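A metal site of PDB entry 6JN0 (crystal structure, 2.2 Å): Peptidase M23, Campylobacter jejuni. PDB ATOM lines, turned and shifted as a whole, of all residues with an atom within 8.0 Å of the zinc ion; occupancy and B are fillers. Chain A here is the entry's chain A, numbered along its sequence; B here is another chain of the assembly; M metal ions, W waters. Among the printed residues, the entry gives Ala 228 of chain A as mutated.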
ATOM      1  N   THR A 132     -18.235 -19.237   1.571  1.00  0.00           N
ATOM      2  CA  THR A 132     -18.909 -17.945   1.413  1.00  0.00           C
ATOM      3  C   THR A 132     -19.831 -17.902   0.216  1.00  0.00           C
ATOM      4  O   THR A 132     -20.659 -16.984   0.135  1.00  0.00           O
ATOM      5  CB  THR A 132     -17.889 -16.807   1.252  1.00  0.00           C
ATOM      6  OG1 THR A 132     -17.055 -17.107   0.133  1.00  0.00           O
ATOM      7  CG2 THR A 132     -17.027 -16.705   2.469  1.00  0.00           C
ATOM      8  N   SER A 133     -19.728 -18.842  -0.713  1.00  0.00           N
ATOM      9  CA  SER A 133     -20.701 -18.899  -1.802  1.00  0.00           C
ATOM     10  C   SER A 133     -20.905 -20.354  -2.191  1.00  0.00           C
ATOM     11  O   SER A 133     -19.968 -21.007  -2.656  1.00  0.00           O
ATOM     12  CB  SER A 133     -20.239 -18.047  -2.987  1.00  0.00           C
ATOM     13  OG  SER A 133     -21.180 -18.082  -4.033  1.00  0.00           O
ATOM     14  N   ASP A 134     -22.131 -20.854  -2.003  1.00  0.00           N
ATOM     15  CA  ASP A 134     -22.435 -22.278  -2.146  1.00  0.00           C
ATOM     16  C   ASP A 134     -22.450 -22.714  -3.604  1.00  0.00           C
ATOM     17  O   ASP A 134     -22.765 -21.932  -4.510  1.00  0.00           O
ATOM     18  CB  ASP A 134     -23.802 -22.626  -1.553  1.00  0.00           C
ATOM     19  CG  ASP A 134     -23.902 -22.394  -0.063  1.00  0.00           C
ATOM     20  OD1 ASP A 134     -22.868 -22.139   0.588  1.00  0.00           O
ATOM     21  OD2 ASP A 134     -25.033 -22.503   0.477  1.00  0.00           O
ATOM     22  N   PHE A 135     -22.156 -23.988  -3.805  1.00  0.00           N
ATOM     23  CA  PHE A 135     -22.367 -24.603  -5.106  1.00  0.00           C
ATOM     24  C   PHE A 135     -23.840 -24.561  -5.481  1.00  0.00           C
ATOM     25  O   PHE A 135     -24.714 -24.758  -4.643  1.00  0.00           O
ATOM     26  CB  PHE A 135     -21.892 -26.060  -5.059  1.00  0.00           C
ATOM     27  CG  PHE A 135     -22.254 -26.845  -6.289  1.00  0.00           C
ATOM     28  CD1 PHE A 135     -23.451 -27.535  -6.369  1.00  0.00           C
ATOM     29  CD2 PHE A 135     -21.374 -26.933  -7.359  1.00  0.00           C
ATOM     30  CE1 PHE A 135     -23.771 -28.268  -7.490  1.00  0.00           C
ATOM     31  CE2 PHE A 135     -21.684 -27.673  -8.472  1.00  0.00           C
ATOM     32  CZ  PHE A 135     -22.882 -28.345  -8.535  1.00  0.00           C
ATOM     33  N   LYS A 137     -25.802 -22.127  -6.723  1.00  0.00           N
ATOM     34  CA  LYS A 137     -26.555 -20.881  -6.820  1.00  0.00           C
ATOM     35  C   LYS A 137     -26.805 -20.598  -8.286  1.00  0.00           C
ATOM     36  O   LYS A 137     -25.870 -20.556  -9.091  1.00  0.00           O
ATOM     37  CB  LYS A 137     -25.779 -19.727  -6.186  1.00  0.00           C
ATOM     38  CG  LYS A 137     -25.421 -19.947  -4.724  1.00  0.00           C
ATOM     39  CD  LYS A 137     -24.159 -19.167  -4.348  1.00  0.00           C
ATOM     40  CE  LYS A 137     -24.488 -17.725  -3.956  1.00  0.00           C
ATOM     41  NZ  LYS A 137     -24.627 -17.569  -2.481  1.00  0.00           N
ATOM     42  N   TYR A 148     -25.026 -21.053 -13.367  1.00  0.00           N
ATOM     43  CA  TYR A 148     -24.964 -21.498 -11.985  1.00  0.00           C
ATOM     44  C   TYR A 148     -23.527 -21.530 -11.502  1.00  0.00           C
ATOM     45  O   TYR A 148     -22.574 -21.535 -12.292  1.00  0.00           O
ATOM     46  CB  TYR A 148     -25.630 -22.868 -11.801  1.00  0.00           C
ATOM     47  CG  TYR A 148     -24.810 -24.044 -12.315  1.00  0.00           C
ATOM     48  CD1 TYR A 148     -24.746 -24.335 -13.681  1.00  0.00           C
ATOM     49  CD2 TYR A 148     -24.124 -24.870 -11.438  1.00  0.00           C
ATOM     50  CE1 TYR A 148     -23.988 -25.432 -14.151  1.00  0.00           C
ATOM     51  CE2 TYR A 148     -23.376 -25.952 -11.895  1.00  0.00           C
ATOM     52  CZ  TYR A 148     -23.303 -26.222 -13.241  1.00  0.00           C
ATOM     53  OH  TYR A 148     -22.562 -27.315 -13.673  1.00  0.00           O
ATOM     54  N   HIS A 149     -23.380 -21.528 -10.188  1.00  0.00           N
ATOM     55  CA  HIS A 149     -22.080 -21.607  -9.532  1.00  0.00           C
ATOM     56  C   HIS A 149     -21.647 -23.070  -9.516  1.00  0.00           C
ATOM     57  O   HIS A 149     -22.212 -23.875  -8.784  1.00  0.00           O
ATOM     58  CB  HIS A 149     -22.179 -21.048  -8.120  1.00  0.00           C
ATOM     59  CG  HIS A 149     -20.850 -20.854  -7.470  1.00  0.00           C
ATOM     60  ND1 HIS A 149     -20.688 -20.904  -6.105  1.00  0.00           N
ATOM     61  CD2 HIS A 149     -19.635 -20.587  -7.992  1.00  0.00           C
ATOM     62  CE1 HIS A 149     -19.421 -20.673  -5.812  1.00  0.00           C
ATOM     63  NE2 HIS A 149     -18.761 -20.487  -6.935  1.00  0.00           N
ATOM     64  N   SER A 150     -20.644 -23.404 -10.320  1.00  0.00           N
ATOM     65  CA  SER A 150     -20.250 -24.784 -10.559  1.00  0.00           C
ATOM     66  C   SER A 150     -19.185 -25.270  -9.582  1.00  0.00           C
ATOM     67  O   SER A 150     -18.566 -26.299  -9.840  1.00  0.00           O
ATOM     68  CB  SER A 150     -19.736 -24.943 -11.994  1.00  0.00           C
ATOM     69  OG  SER A 150     -18.497 -24.245 -12.157  1.00  0.00           O
ATOM     70  N   GLY A 151     -18.922 -24.533  -8.516  1.00  0.00           N
ATOM     71  CA  GLY A 151     -18.048 -24.986  -7.447  1.00  0.00           C
ATOM     72  C   GLY A 151     -18.451 -24.337  -6.144  1.00  0.00           C
ATOM     73  O   GLY A 151     -19.525 -23.710  -6.086  1.00  0.00           O
ATOM     74  N   THR A 152     -17.640 -24.427  -5.106  1.00  0.00           N
ATOM     75  CA  THR A 152     -17.922 -23.734  -3.853  1.00  0.00           C
ATOM     76  C   THR A 152     -16.757 -22.817  -3.520  1.00  0.00           C
ATOM     77  O   THR A 152     -15.603 -23.168  -3.762  1.00  0.00           O
ATOM     78  CB  THR A 152     -18.205 -24.739  -2.730  1.00  0.00           C
ATOM     79  OG1 THR A 152     -18.604 -24.026  -1.557  1.00  0.00           O
ATOM     80  CG2 THR A 152     -16.976 -25.588  -2.397  1.00  0.00           C
ATOM     81  N   ASP A 153     -17.062 -21.623  -2.996  1.00  0.00           N
ATOM     82  CA  ASP A 153     -16.055 -20.620  -2.659  1.00  0.00           C
ATOM     83  C   ASP A 153     -15.764 -20.646  -1.164  1.00  0.00           C
ATOM     84  O   ASP A 153     -16.680 -20.521  -0.354  1.00  0.00           O
ATOM     85  CB  ASP A 153     -16.524 -19.201  -3.046  1.00  0.00           C
ATOM     86  CG  ASP A 153     -16.622 -19.009  -4.551  1.00  0.00           C
ATOM     87  OD1 ASP A 153     -16.159 -19.904  -5.275  1.00  0.00           O
ATOM     88  OD2 ASP A 153     -17.182 -17.985  -4.999  1.00  0.00           O
ATOM     89  N   PHE A 154     -14.476 -20.759  -0.835  1.00  0.00           N
ATOM     90  CA  PHE A 154     -13.981 -20.627   0.526  1.00  0.00           C
ATOM     91  C   PHE A 154     -13.489 -19.213   0.759  1.00  0.00           C
ATOM     92  O   PHE A 154     -12.885 -18.603  -0.129  1.00  0.00           O
ATOM     93  CB  PHE A 154     -12.789 -21.564   0.791  1.00  0.00           C
ATOM     94  CG  PHE A 154     -13.160 -23.021   0.912  1.00  0.00           C
ATOM     95  CD1 PHE A 154     -13.425 -23.767  -0.224  1.00  0.00           C
ATOM     96  CD2 PHE A 154     -13.192 -23.638   2.145  1.00  0.00           C
ATOM     97  CE1 PHE A 154     -13.735 -25.138  -0.117  1.00  0.00           C
ATOM     98  CE2 PHE A 154     -13.492 -25.015   2.260  1.00  0.00           C
ATOM     99  CZ  PHE A 154     -13.772 -25.751   1.125  1.00  0.00           C
ATOM    100  N   TYR A 196      -9.334 -22.549  -8.290  1.00  0.00           N
ATOM    101  CA  TYR A 196      -9.366 -21.431  -9.238  1.00  0.00           C
ATOM    102  C   TYR A 196      -9.127 -20.080  -8.541  1.00  0.00           C
ATOM    103  O   TYR A 196      -9.285 -19.942  -7.331  1.00  0.00           O
ATOM    104  CB  TYR A 196     -10.699 -21.383  -9.983  1.00  0.00           C
ATOM    105  CG  TYR A 196     -10.967 -22.538 -10.927  1.00  0.00           C
ATOM    106  CD1 TYR A 196      -9.974 -23.442 -11.253  1.00  0.00           C
ATOM    107  CD2 TYR A 196     -12.236 -22.712 -11.493  1.00  0.00           C
ATOM    108  CE1 TYR A 196     -10.219 -24.508 -12.123  1.00  0.00           C
ATOM    109  CE2 TYR A 196     -12.480 -23.778 -12.363  1.00  0.00           C
ATOM    110  CZ  TYR A 196     -11.465 -24.672 -12.670  1.00  0.00           C
ATOM    111  OH  TYR A 196     -11.686 -25.737 -13.517  1.00  0.00           O
ATOM    112  N   HIS A 197      -8.731 -19.088  -9.362  1.00  0.00           N
ATOM    113  CA  HIS A 197      -8.568 -17.681  -8.976  1.00  0.00           C
ATOM    114  C   HIS A 197      -7.310 -17.450  -8.151  1.00  0.00           C
ATOM    115  O   HIS A 197      -7.205 -16.419  -7.459  1.00  0.00           O
ATOM    116  CB  HIS A 197      -9.781 -17.139  -8.230  1.00  0.00           C
ATOM    117  CG  HIS A 197     -11.080 -17.417  -8.927  1.00  0.00           C
ATOM    118  ND1 HIS A 197     -11.276 -17.126 -10.260  1.00  0.00           N
ATOM    119  CD2 HIS A 197     -12.218 -17.999  -8.493  1.00  0.00           C
ATOM    120  CE1 HIS A 197     -12.484 -17.521 -10.614  1.00  0.00           C
ATOM    121  NE2 HIS A 197     -13.078 -18.048  -9.563  1.00  0.00           N
ATOM    122  N   ARG A 223     -11.377 -13.122 -11.144  1.00  0.00           N
ATOM    123  CA  ARG A 223     -12.513 -13.004 -10.230  1.00  0.00           C
ATOM    124  C   ARG A 223     -12.911 -11.536 -10.063  1.00  0.00           C
ATOM    125  O   ARG A 223     -12.063 -10.673  -9.790  1.00  0.00           O
ATOM    126  CB  ARG A 223     -12.207 -13.622  -8.868  1.00  0.00           C
ATOM    127  CG  ARG A 223     -13.461 -14.082  -8.126  1.00  0.00           C
ATOM    128  CD  ARG A 223     -13.171 -15.057  -7.004  1.00  0.00           C
ATOM    129  NE  ARG A 223     -14.384 -15.521  -6.358  1.00  0.00           N
ATOM    130  CZ  ARG A 223     -14.974 -14.919  -5.325  1.00  0.00           C
ATOM    131  NH1 ARG A 223     -14.457 -13.811  -4.818  1.00  0.00           N
ATOM    132  NH2 ARG A 223     -16.085 -15.431  -4.786  1.00  0.00           N
ATOM    133  N   ALA A 228     -11.015 -15.004  -3.193  1.00  0.00           N
ATOM    134  CA  ALA A 228     -11.603 -16.230  -2.643  1.00  0.00           C
ATOM    135  C   ALA A 228     -10.928 -17.420  -3.310  1.00  0.00           C
ATOM    136  O   ALA A 228     -10.247 -17.272  -4.324  1.00  0.00           O
ATOM    137  CB  ALA A 228     -13.126 -16.287  -2.862  1.00  0.00           C
ATOM    138  N   LEU A 229     -11.155 -18.605  -2.744  1.00  0.00           N
ATOM    139  CA  LEU A 229     -10.755 -19.869  -3.370  1.00  0.00           C
ATOM    140  C   LEU A 229     -12.014 -20.542  -3.905  1.00  0.00           C
ATOM    141  O   LEU A 229     -12.916 -20.876  -3.124  1.00  0.00           O
ATOM    142  CB  LEU A 229     -10.022 -20.786  -2.386  1.00  0.00           C
ATOM    143  CG  LEU A 229      -9.305 -22.096  -2.807  1.00  0.00           C
ATOM    144  CD1 LEU A 229     -10.232 -23.329  -2.834  1.00  0.00           C
ATOM    145  CD2 LEU A 229      -8.537 -21.982  -4.143  1.00  0.00           C
ATOM    146  N   HIS A 230     -12.074 -20.753  -5.212  1.00  0.00           N
ATOM    147  CA  HIS A 230     -13.144 -21.526  -5.814  1.00  0.00           C
ATOM    148  C   HIS A 230     -12.665 -22.964  -5.927  1.00  0.00           C
ATOM    149  O   HIS A 230     -11.638 -23.225  -6.567  1.00  0.00           O
ATOM    150  CB  HIS A 230     -13.528 -20.948  -7.176  1.00  0.00           C
ATOM    151  CG  HIS A 230     -14.344 -21.863  -8.032  1.00  0.00           C
ATOM    152  ND1 HIS A 230     -15.662 -21.634  -8.338  1.00  0.00           N
ATOM    153  CD2 HIS A 230     -14.011 -23.019  -8.675  1.00  0.00           C
ATOM    154  CE1 HIS A 230     -16.117 -22.585  -9.124  1.00  0.00           C
ATOM    155  NE2 HIS A 230     -15.127 -23.451  -9.336  1.00  0.00           N
ATOM    156  N   PHE A 231     -13.397 -23.888  -5.306  1.00  0.00           N
ATOM    157  CA  PHE A 231     -13.044 -25.304  -5.291  1.00  0.00           C
ATOM    158  C   PHE A 231     -14.120 -26.085  -6.035  1.00  0.00           C
ATOM    159  O   PHE A 231     -15.306 -25.953  -5.736  1.00  0.00           O
ATOM    160  CB  PHE A 231     -12.901 -25.788  -3.839  1.00  0.00           C
ATOM    161  CG  PHE A 231     -12.635 -27.278  -3.697  1.00  0.00           C
ATOM    162  CD1 PHE A 231     -11.414 -27.825  -4.080  1.00  0.00           C
ATOM    163  CD2 PHE A 231     -13.605 -28.123  -3.147  1.00  0.00           C
ATOM    164  CE1 PHE A 231     -11.152 -29.200  -3.925  1.00  0.00           C
ATOM    165  CE2 PHE A 231     -13.355 -29.505  -2.984  1.00  0.00           C
ATOM    166  CZ  PHE A 231     -12.128 -30.032  -3.395  1.00  0.00           C
ATOM    167  N   GLY A 232     -13.697 -26.888  -7.018  1.00  0.00           N
ATOM    168  CA  GLY A 232     -14.641 -27.659  -7.793  1.00  0.00           C
ATOM    169  C   GLY A 232     -14.263 -29.127  -7.828  1.00  0.00           C
ATOM    170  O   GLY A 232     -13.105 -29.505  -7.605  1.00  0.00           O
ATOM    171  C   C0O B   1     -15.397 -20.955 -13.869  1.00  0.00           C
ATOM    172  CA  C0O B   1     -15.717 -22.057 -14.883  1.00  0.00           C
ATOM    173  C3  C0O B   1     -14.436 -22.319 -15.678  1.00  0.00           C
ATOM    174  C4  C0O B   1     -14.644 -22.628 -17.155  1.00  0.00           C
ATOM    175  C5  C0O B   1     -13.634 -23.653 -17.688  1.00  0.00           C
ATOM    176  C6  C0O B   1     -14.101 -25.072 -17.359  1.00  0.00           C
ATOM    177  C7  C0O B   1     -13.174 -25.710 -16.298  1.00  0.00           C
ATOM    178  O   C0O B   1     -14.324 -20.465 -13.896  1.00  0.00           O
ATOM    179  O3  C0O B   1     -12.117 -26.298 -16.690  1.00  0.00           O
ATOM    180  O4  C0O B   1     -13.618 -25.562 -15.133  1.00  0.00           O
ATOM    181  N   C0O B   1     -16.793 -21.605 -15.758  1.00  0.00           N
ATOM    182  N6  C0O B   1     -14.206 -25.864 -18.583  1.00  0.00           N
ATOM    183  N   DAL B   2     -16.390 -20.478 -12.913  1.00  0.00           N
ATOM    184  CA  DAL B   2     -16.021 -19.420 -11.987  1.00  0.00           C
ATOM    185  CB  DAL B   2     -14.996 -19.973 -11.004  1.00  0.00           C
ATOM    186  C   DAL B   2     -17.227 -18.943 -11.189  1.00  0.00           C
ATOM    187  O   DAL B   2     -17.364 -19.359 -10.076  1.00  0.00           O
ATOM    188  C   API B   3     -15.489 -14.240 -11.450  1.00  0.00           C
ATOM    189  CA  API B   3     -16.244 -14.484 -10.140  1.00  0.00           C
ATOM    190  C3  API B   3     -17.630 -15.089 -10.386  1.00  0.00           C
ATOM    191  C4  API B   3     -17.933 -16.185  -9.370  1.00  0.00           C
ATOM    192  C5  API B   3     -19.195 -16.990  -9.677  1.00  0.00           C
ATOM    193  C6  API B   3     -19.364 -17.413 -11.149  1.00  0.00           C
ATOM    194  C7  API B   3     -20.548 -18.382 -11.293  1.00  0.00           C
ATOM    195  O   API B   3     -15.039 -15.253 -12.064  1.00  0.00           O
ATOM    196  OXT API B   3     -15.405 -13.035 -11.765  1.00  0.00           O
ATOM    197  O3  API B   3     -20.481 -19.040 -12.373  1.00  0.00           O
ATOM    198  O4  API B   3     -21.364 -18.314 -10.337  1.00  0.00           O
ATOM    199  N   API B   3     -16.350 -13.210  -9.448  1.00  0.00           N
ATOM    200  N6  API B   3     -18.160 -17.988 -11.768  1.00  0.00           N
HETATM  201 ZN    ZN M   1     -16.774 -20.048  -7.170  1.00  0.00          ZN
HETATM  202  O   HOH W   1     -15.747 -18.048  -7.993  1.00  0.00           O
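O of Gly 151 lies within hydrogen-bond range of ND1 of His 149 (3.0 Å). N of His 149 sits at hydrogen-bond distance from O of Lys 137 (2.9 Å). ND1 of His 149 sits at hydrogen-bond distance from O of Asp 134, 2.8 Å away. O of Asp 153 is in hydrogen-bond range of N of Thr 132 (2.8 Å). N of Asp 153 sits at hydrogen-bond distance from O of Ser 133, at 3.0 Å. O of His 230 is in hydrogen-bond range of N of Tyr 196 (3.0 Å). A ring nitrogen (ND1) of His 230 sits close to O of DAL 2 of chain B. The side-chain carboxylate (OD2) of Asp 153 is in salt-bridge range of the guanidinium group (NH2) of Arg 223 (2.8 Å).
Merely in contact with the zinc ion: DAL 2 of chain B (3.0 Å). Of the 23 residues printed, 4 come within 4 Å of the zinc ion.
The zinc ion is bound by OD1 of Asp 153, NE2 of His 149, ND1 of His 230 and water W1. The zinc ion has four donor atoms within binding distance.
Water W1 lies within hydrogen-bond range of O of DAL 2 of chain B, NE2 of His 197, NE of Arg 223 and OD2 of Asp 153.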
